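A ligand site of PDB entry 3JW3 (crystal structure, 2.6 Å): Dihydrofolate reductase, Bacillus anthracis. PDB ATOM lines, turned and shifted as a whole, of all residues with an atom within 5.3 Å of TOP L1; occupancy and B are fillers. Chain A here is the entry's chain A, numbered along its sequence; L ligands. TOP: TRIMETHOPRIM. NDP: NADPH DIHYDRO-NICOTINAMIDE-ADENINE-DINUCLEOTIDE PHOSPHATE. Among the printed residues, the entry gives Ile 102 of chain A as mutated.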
ATOM      1  N   MET A  12     -32.511   9.404  17.320  1.00  0.00           N
ATOM      2  CA  MET A  12     -31.523  10.350  16.816  1.00  0.00           C
ATOM      3  C   MET A  12     -30.968   9.780  15.520  1.00  0.00           C
ATOM      4  O   MET A  12     -30.285   8.747  15.523  1.00  0.00           O
ATOM      5  CB  MET A  12     -30.398  10.533  17.828  1.00  0.00           C
ATOM      6  CG  MET A  12     -29.248  11.374  17.333  1.00  0.00           C
ATOM      7  SD  MET A  12     -29.688  13.103  17.162  1.00  0.00           S
ATOM      8  CE  MET A  12     -30.279  13.531  18.796  1.00  0.00           C
ATOM      9  N   VAL A  13     -31.277  10.436  14.412  1.00  0.00           N
ATOM     10  CA  VAL A  13     -30.887   9.925  13.109  1.00  0.00           C
ATOM     11  C   VAL A  13     -30.464  11.037  12.160  1.00  0.00           C
ATOM     12  O   VAL A  13     -30.972  12.162  12.245  1.00  0.00           O
ATOM     13  CB  VAL A  13     -32.012   9.000  12.501  1.00  0.00           C
ATOM     14  CG1 VAL A  13     -33.383   9.590  12.687  1.00  0.00           C
ATOM     15  CG2 VAL A  13     -31.741   8.679  11.018  1.00  0.00           C
ATOM     16  N   ALA A  14     -29.499  10.718  11.299  1.00  0.00           N
ATOM     17  CA  ALA A  14     -29.165  11.541  10.145  1.00  0.00           C
ATOM     18  C   ALA A  14     -29.308  10.690   8.880  1.00  0.00           C
ATOM     19  O   ALA A  14     -28.735   9.610   8.795  1.00  0.00           O
ATOM     20  CB  ALA A  14     -27.767  12.091  10.285  1.00  0.00           C
ATOM     21  N   LEU A  27     -20.736   6.181   7.987  1.00  0.00           N
ATOM     22  CA  LEU A  27     -21.434   7.369   7.515  1.00  0.00           C
ATOM     23  C   LEU A  27     -20.908   7.719   6.117  1.00  0.00           C
ATOM     24  O   LEU A  27     -19.703   7.916   5.939  1.00  0.00           O
ATOM     25  CB  LEU A  27     -21.192   8.531   8.471  1.00  0.00           C
ATOM     26  CG  LEU A  27     -22.302   8.999   9.415  1.00  0.00           C
ATOM     27  CD1 LEU A  27     -23.227   7.880   9.869  1.00  0.00           C
ATOM     28  CD2 LEU A  27     -21.657   9.700  10.604  1.00  0.00           C
ATOM     29  N   GLU A  34     -22.537  18.207  12.462  1.00  0.00           N
ATOM     30  CA  GLU A  34     -23.738  17.420  12.700  1.00  0.00           C
ATOM     31  C   GLU A  34     -23.512  16.546  13.903  1.00  0.00           C
ATOM     32  O   GLU A  34     -24.405  16.379  14.742  1.00  0.00           O
ATOM     33  CB  GLU A  34     -24.089  16.550  11.487  1.00  0.00           C
ATOM     34  CG  GLU A  34     -25.575  16.245  11.364  1.00  0.00           C
ATOM     35  CD  GLU A  34     -26.052  15.111  12.262  1.00  0.00           C
ATOM     36  OE1 GLU A  34     -25.268  14.150  12.447  1.00  0.00           O
ATOM     37  OE2 GLU A  34     -27.212  15.178  12.770  1.00  0.00           O
ATOM     38  N   LEU A  35     -22.311  15.998  14.007  1.00  0.00           N
ATOM     39  CA  LEU A  35     -21.936  15.188  15.154  1.00  0.00           C
ATOM     40  C   LEU A  35     -21.897  16.023  16.416  1.00  0.00           C
ATOM     41  O   LEU A  35     -22.202  15.503  17.490  1.00  0.00           O
ATOM     42  CB  LEU A  35     -20.622  14.441  14.935  1.00  0.00           C
ATOM     43  CG  LEU A  35     -20.579  13.535  13.699  1.00  0.00           C
ATOM     44  CD1 LEU A  35     -19.224  12.845  13.559  1.00  0.00           C
ATOM     45  CD2 LEU A  35     -21.706  12.510  13.714  1.00  0.00           C
ATOM     46  N   VAL A  38     -25.387  16.345  17.706  1.00  0.00           N
ATOM     47  CA  VAL A  38     -25.783  15.086  18.352  1.00  0.00           C
ATOM     48  C   VAL A  38     -25.242  15.058  19.762  1.00  0.00           C
ATOM     49  O   VAL A  38     -25.963  14.678  20.698  1.00  0.00           O
ATOM     50  CB  VAL A  38     -25.317  13.843  17.560  1.00  0.00           C
ATOM     51  CG1 VAL A  38     -25.511  12.574  18.395  1.00  0.00           C
ATOM     52  CG2 VAL A  38     -26.071  13.722  16.265  1.00  0.00           C
ATOM     53  N   LEU A  47     -27.222   6.438  25.503  1.00  0.00           N
ATOM     54  CA  LEU A  47     -27.223   6.170  24.081  1.00  0.00           C
ATOM     55  C   LEU A  47     -27.434   4.672  23.884  1.00  0.00           C
ATOM     56  O   LEU A  47     -26.682   3.858  24.430  1.00  0.00           O
ATOM     57  CB  LEU A  47     -25.900   6.579  23.453  1.00  0.00           C
ATOM     58  CG  LEU A  47     -25.608   7.989  22.969  1.00  0.00           C
ATOM     59  CD1 LEU A  47     -26.573   9.038  23.505  1.00  0.00           C
ATOM     60  CD2 LEU A  47     -24.146   8.331  23.283  1.00  0.00           C
ATOM     61  N   ASN A  53     -23.524  -0.866  14.912  1.00  0.00           N
ATOM     62  CA  ASN A  53     -23.372   0.587  15.051  1.00  0.00           C
ATOM     63  C   ASN A  53     -22.259   0.921  16.031  1.00  0.00           C
ATOM     64  O   ASN A  53     -21.459   1.817  15.749  1.00  0.00           O
ATOM     65  CB  ASN A  53     -24.680   1.248  15.483  1.00  0.00           C
ATOM     66  CG  ASN A  53     -24.644   2.780  15.331  1.00  0.00           C
ATOM     67  OD1 ASN A  53     -23.946   3.314  14.459  1.00  0.00           O
ATOM     68  ND2 ASN A  53     -25.404   3.479  16.166  1.00  0.00           N
ATOM     69  N   ALA A  56     -18.632   0.095  14.505  1.00  0.00           N
ATOM     70  CA  ALA A  56     -18.310   1.093  13.499  1.00  0.00           C
ATOM     71  C   ALA A  56     -17.966   2.440  14.138  1.00  0.00           C
ATOM     72  O   ALA A  56     -17.190   3.199  13.580  1.00  0.00           O
ATOM     73  CB  ALA A  56     -19.427   1.257  12.495  1.00  0.00           C
ATOM     74  N   ILE A  57     -18.564   2.726  15.296  1.00  0.00           N
ATOM     75  CA  ILE A  57     -18.157   3.895  16.111  1.00  0.00           C
ATOM     76  C   ILE A  57     -16.803   3.659  16.836  1.00  0.00           C
ATOM     77  O   ILE A  57     -15.995   4.579  16.955  1.00  0.00           O
ATOM     78  CB  ILE A  57     -19.268   4.367  17.100  1.00  0.00           C
ATOM     79  CG1 ILE A  57     -20.482   4.897  16.339  1.00  0.00           C
ATOM     80  CG2 ILE A  57     -18.741   5.463  18.035  1.00  0.00           C
ATOM     81  CD1 ILE A  57     -21.781   5.024  17.165  1.00  0.00           C
ATOM     82  N   LEU A  61     -18.383   6.860  24.185  1.00  0.00           N
ATOM     83  CA  LEU A  61     -18.278   8.318  24.123  1.00  0.00           C
ATOM     84  C   LEU A  61     -18.737   8.977  25.422  1.00  0.00           C
ATOM     85  O   LEU A  61     -19.890   8.804  25.833  1.00  0.00           O
ATOM     86  CB  LEU A  61     -18.964   8.873  22.862  1.00  0.00           C
ATOM     87  CG  LEU A  61     -18.408   8.286  21.532  1.00  0.00           C
ATOM     88  CD1 LEU A  61     -19.419   8.412  20.397  1.00  0.00           C
ATOM     89  CD2 LEU A  61     -17.014   8.860  21.110  1.00  0.00           C
ATOM     90  N   ILE A 101     -32.007   6.513  20.948  1.00  0.00           N
ATOM     91  CA  ILE A 101     -31.758   5.399  20.063  1.00  0.00           C
ATOM     92  C   ILE A 101     -30.975   5.929  18.866  1.00  0.00           C
ATOM     93  O   ILE A 101     -31.530   6.655  18.040  1.00  0.00           O
ATOM     94  CB  ILE A 101     -33.081   4.782  19.571  1.00  0.00           C
ATOM     95  CG1 ILE A 101     -34.088   4.660  20.738  1.00  0.00           C
ATOM     96  CG2 ILE A 101     -32.835   3.462  18.828  1.00  0.00           C
ATOM     97  CD1 ILE A 101     -33.763   3.583  21.749  1.00  0.00           C
ATOM     98  N   ILE A 102     -29.704   5.576  18.782  1.00  0.00           N
ATOM     99  CA  ILE A 102     -28.843   6.189  17.778  1.00  0.00           C
ATOM    100  C   ILE A 102     -28.474   5.261  16.611  1.00  0.00           C
ATOM    101  O   ILE A 102     -27.580   5.581  15.835  1.00  0.00           O
ATOM    102  CB  ILE A 102     -27.594   6.862  18.430  1.00  0.00           C
ATOM    103  CG1 ILE A 102     -26.720   5.839  19.145  1.00  0.00           C
ATOM    104  CG2 ILE A 102     -28.002   7.981  19.387  1.00  0.00           C
ATOM    105  CD1 ILE A 102     -25.254   6.254  19.208  1.00  0.00           C
ATOM    106  N   GLY A 103     -29.177   4.132  16.489  1.00  0.00           N
ATOM    107  CA  GLY A 103     -28.973   3.226  15.350  1.00  0.00           C
ATOM    108  C   GLY A 103     -28.217   1.947  15.649  1.00  0.00           C
ATOM    109  O   GLY A 103     -27.756   1.741  16.779  1.00  0.00           O
ATOM    110  N   TYR A 108     -33.146   0.492  15.087  1.00  0.00           N
ATOM    111  CA  TYR A 108     -34.283   1.377  14.839  1.00  0.00           C
ATOM    112  C   TYR A 108     -35.585   0.589  14.724  1.00  0.00           C
ATOM    113  O   TYR A 108     -36.580   0.957  15.341  1.00  0.00           O
ATOM    114  CB  TYR A 108     -34.075   2.262  13.614  1.00  0.00           C
ATOM    115  CG  TYR A 108     -33.071   3.374  13.784  1.00  0.00           C
ATOM    116  CD1 TYR A 108     -33.142   4.241  14.865  1.00  0.00           C
ATOM    117  CD2 TYR A 108     -32.070   3.587  12.843  1.00  0.00           C
ATOM    118  CE1 TYR A 108     -32.226   5.269  15.027  1.00  0.00           C
ATOM    119  CE2 TYR A 108     -31.161   4.605  12.985  1.00  0.00           C
ATOM    120  CZ  TYR A 108     -31.241   5.446  14.073  1.00  0.00           C
ATOM    121  OH  TYR A 108     -30.325   6.458  14.201  1.00  0.00           O
ATOM    122  N   TYR A 119     -35.580  13.016  16.215  1.00  0.00           N
ATOM    123  CA  TYR A 119     -34.541  13.978  15.796  1.00  0.00           C
ATOM    124  C   TYR A 119     -33.877  13.486  14.521  1.00  0.00           C
ATOM    125  O   TYR A 119     -32.960  12.661  14.566  1.00  0.00           O
ATOM    126  CB  TYR A 119     -33.485  14.137  16.867  1.00  0.00           C
ATOM    127  CG  TYR A 119     -33.943  14.729  18.180  1.00  0.00           C
ATOM    128  CD1 TYR A 119     -34.518  13.931  19.176  1.00  0.00           C
ATOM    129  CD2 TYR A 119     -33.761  16.098  18.441  1.00  0.00           C
ATOM    130  CE1 TYR A 119     -34.912  14.467  20.378  1.00  0.00           C
ATOM    131  CE2 TYR A 119     -34.162  16.641  19.658  1.00  0.00           C
ATOM    132  CZ  TYR A 119     -34.728  15.817  20.627  1.00  0.00           C
ATOM    133  OH  TYR A 119     -35.111  16.335  21.836  1.00  0.00           O
ATOM    134  N   THR A 121     -31.923  14.459  11.061  1.00  0.00           N
ATOM    135  CA  THR A 121     -31.200  15.383  10.221  1.00  0.00           C
ATOM    136  C   THR A 121     -31.408  14.912   8.788  1.00  0.00           C
ATOM    137  O   THR A 121     -31.078  13.761   8.459  1.00  0.00           O
ATOM    138  CB  THR A 121     -29.696  15.426  10.546  1.00  0.00           C
ATOM    139  OG1 THR A 121     -29.503  15.861  11.898  1.00  0.00           O
ATOM    140  CG2 THR A 121     -28.977  16.366   9.595  1.00  0.00           C
HETATM  141  C1  TOP L   1     -25.123  10.442  13.626  1.00  0.00           C
HETATM  142  N2  TOP L   1     -25.912  11.532  13.497  1.00  0.00           N
HETATM  143  C3  TOP L   1     -27.217  11.518  13.846  1.00  0.00           C
HETATM  144  N4  TOP L   1     -27.961  12.630  13.681  1.00  0.00           N
HETATM  145  N5  TOP L   1     -27.795  10.398  14.357  1.00  0.00           N
HETATM  146  C6  TOP L   1     -27.073   9.266  14.534  1.00  0.00           C
HETATM  147  N7  TOP L   1     -27.643   8.149  15.040  1.00  0.00           N
HETATM  148  C8  TOP L   1     -25.636   9.247  14.151  1.00  0.00           C
HETATM  149  C9  TOP L   1     -24.807   7.979  14.344  1.00  0.00           C
HETATM  150  C10 TOP L   1     -23.407   8.319  14.793  1.00  0.00           C
HETATM  151  C11 TOP L   1     -23.249   9.171  15.880  1.00  0.00           C
HETATM  152  C12 TOP L   1     -21.993   9.554  16.346  1.00  0.00           C
HETATM  153  O13 TOP L   1     -21.914  10.401  17.418  1.00  0.00           O
HETATM  154  C14 TOP L   1     -22.339   9.985  18.720  1.00  0.00           C
HETATM  155  C15 TOP L   1     -20.764   9.026  15.646  1.00  0.00           C
HETATM  156  O16 TOP L   1     -19.520   9.388  16.141  1.00  0.00           O
HETATM  157  C17 TOP L   1     -18.337   9.621  15.354  1.00  0.00           C
HETATM  158  C18 TOP L   1     -20.969   8.082  14.484  1.00  0.00           C
HETATM  159  O19 TOP L   1     -19.888   7.542  13.794  1.00  0.00           O
HETATM  160  C20 TOP L   1     -20.026   6.408  12.895  1.00  0.00           C
HETATM  161  C21 TOP L   1     -22.297   7.778  14.110  1.00  0.00           C
HETATM  162  PA  NDP L   2     -27.187  -2.341  13.988  1.00  0.00           P
HETATM  163  O1A NDP L   2     -28.666  -2.279  14.076  1.00  0.00           O
HETATM  164  O2A NDP L   2     -26.531  -1.118  14.492  1.00  0.00           O
HETATM  165  O5B NDP L   2     -26.605  -3.598  14.759  1.00  0.00           O
HETATM  166  C5B NDP L   2     -27.084  -4.880  14.424  1.00  0.00           C
HETATM  167  C4B NDP L   2     -26.786  -5.769  15.613  1.00  0.00           C
HETATM  168  O4B NDP L   2     -27.674  -5.509  16.684  1.00  0.00           O
HETATM  169  C3B NDP L   2     -26.958  -7.245  15.304  1.00  0.00           C
HETATM  170  O3B NDP L   2     -25.820  -7.773  14.663  1.00  0.00           O
HETATM  171  C2B NDP L   2     -27.138  -7.802  16.697  1.00  0.00           C
HETATM  172  O2B NDP L   2     -25.873  -7.828  17.316  1.00  0.00           O
HETATM  173  C1B NDP L   2     -27.910  -6.711  17.404  1.00  0.00           C
HETATM  174  N9A NDP L   2     -29.348  -7.023  17.368  1.00  0.00           N
HETATM  175  C8A NDP L   2     -30.200  -6.840  16.305  1.00  0.00           C
HETATM  176  N7A NDP L   2     -31.429  -7.236  16.660  1.00  0.00           N
HETATM  177  C5A NDP L   2     -31.382  -7.671  17.943  1.00  0.00           C
HETATM  178  C6A NDP L   2     -32.355  -8.193  18.788  1.00  0.00           C
HETATM  179  N6A NDP L   2     -33.600  -8.305  18.343  1.00  0.00           N
HETATM  180  N1A NDP L   2     -32.034  -8.583  20.075  1.00  0.00           N
HETATM  181  C2A NDP L   2     -30.726  -8.435  20.509  1.00  0.00           C
HETATM  182  N3A NDP L   2     -29.754  -7.923  19.653  1.00  0.00           N
HETATM  183  C4A NDP L   2     -30.079  -7.549  18.391  1.00  0.00           C
HETATM  184  O3  NDP L   2     -26.716  -2.717  12.493  1.00  0.00           O
HETATM  185  PN  NDP L   2     -27.034  -2.187  11.010  1.00  0.00           P
HETATM  186  O1N NDP L   2     -25.958  -2.720  10.131  1.00  0.00           O
HETATM  187  O2N NDP L   2     -28.459  -2.475  10.719  1.00  0.00           O
HETATM  188  O5D NDP L   2     -26.834  -0.600  11.166  1.00  0.00           O
HETATM  189  C5D NDP L   2     -25.540  -0.066  11.303  1.00  0.00           C
HETATM  190  C4D NDP L   2     -25.168   0.721  10.052  1.00  0.00           C
HETATM  191  O4D NDP L   2     -25.914   1.927   9.964  1.00  0.00           O
HETATM  192  C3D NDP L   2     -23.696   1.121  10.022  1.00  0.00           C
HETATM  193  O3D NDP L   2     -23.257   1.041   8.694  1.00  0.00           O
HETATM  194  C2D NDP L   2     -23.691   2.568  10.474  1.00  0.00           C
HETATM  195  O2D NDP L   2     -22.644   3.277   9.833  1.00  0.00           O
HETATM  196  C1D NDP L   2     -25.079   3.074  10.074  1.00  0.00           C
HETATM  197  N1N NDP L   2     -25.704   4.028  11.035  1.00  0.00           N
HETATM  198  C2N NDP L   2     -25.980   5.324  10.645  1.00  0.00           C
HETATM  199  C3N NDP L   2     -26.582   6.257  11.516  1.00  0.00           C
HETATM  200  C7N NDP L   2     -27.258   7.507  10.974  1.00  0.00           C
HETATM  201  O7N NDP L   2     -28.480   7.938  11.560  1.00  0.00           O
HETATM  202  N7N NDP L   2     -26.697   8.184   9.966  1.00  0.00           N
HETATM  203  C4N NDP L   2     -26.904   5.819  12.787  1.00  0.00           C
HETATM  204  C5N NDP L   2     -26.625   4.513  13.175  1.00  0.00           C
HETATM  205  C6N NDP L   2     -26.029   3.611  12.296  1.00  0.00           C
HETATM  206  P2B NDP L   2     -24.971  -9.152  17.349  1.00  0.00           P
HETATM  207  O1X NDP L   2     -25.769 -10.194  18.084  1.00  0.00           O
HETATM  208  O2X NDP L   2     -24.715  -9.642  15.947  1.00  0.00           O
HETATM  209  O3X NDP L   2     -23.666  -8.830  18.038  1.00  0.00           O
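A nitrogen (N7) of TOP L1 lies within hydrogen-bond range of the backbone carbonyl oxygen (O) of Ile 102 (2.7 Å). The backbone carbonyl oxygen (O) of Met 12 lies within hydrogen-bond range of a nitrogen (N7) of TOP L1, at 2.8 Å. The side-chain carboxylate (OE2) of Glu 34 lies within hydrogen-bond range of a nitrogen (N4) of TOP L1, 2.8 Å away. The side-chain hydroxyl (OH) of Tyr 108 is in hydrogen-bond range of a nitrogen (N7) of TOP L1 (3.3 Å). A nitrogen (N5) of TOP L1 lies close to the backbone NH (N) of Val 13 (3.5 Å). O of Val 13 sits close to N4 of TOP L1, 3.4 Å away. N of Ala 14 lies within hydrogen-bond range of O7N of NDP L2 (3.0 Å). The backbone carbonyl oxygen (O) of Ala 14 is in hydrogen-bond range of a nitrogen (N7N) of NDP L2, 2.7 Å away. The backbone NH (N) of Asn 53 lies within hydrogen-bond range of an oxygen (O2A) of NDP L2.
O of Ile 102 lies close to OH of Tyr 108 (3.3 Å). O of Ile 102 sits at hydrogen-bond distance from ND2 of Asn 53, 3.0 Å away. The backbone carbonyl oxygen of Met 12 is in hydrogen-bond range of the side-chain hydroxyl of Tyr 108, at 2.6 Å. N of Met 12 sits at hydrogen-bond distance from O of Ile 101, 3.0 Å away. The side-chain carboxylate of Glu 34 sits at hydrogen-bond distance from the side-chain hydroxyl of Thr 121 (2.5 Å). The backbone NH (N) of Gly 103 sits close to the side-chain hydroxyl (OH) of Tyr 108, 3.5 Å away. The backbone carbonyl oxygen (O) of Val 13 is in hydrogen-bond range of the backbone NH (N) of Thr 121 (2.8 Å). O of Tyr 119 is in hydrogen-bond range of N of Val 13 (2.8 Å).
A nitrogen (N4) of TOP L1 sits close to the backbone NH of Ala 14 (3.4 Å). Merely in contact with TOP L1: Val 38, Leu 61, Ile 57, Leu 35 and Thr 121. Within 4 Å of TOP L1: Met 12, Val 13, Ala 14, Glu 34, Leu 35, Val 38, Ile 57, Leu 61, Ile 102, Tyr 108 and Thr 121. The nearest printed residue that does not touch TOP L1 is Leu 27 (4.05 Å).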
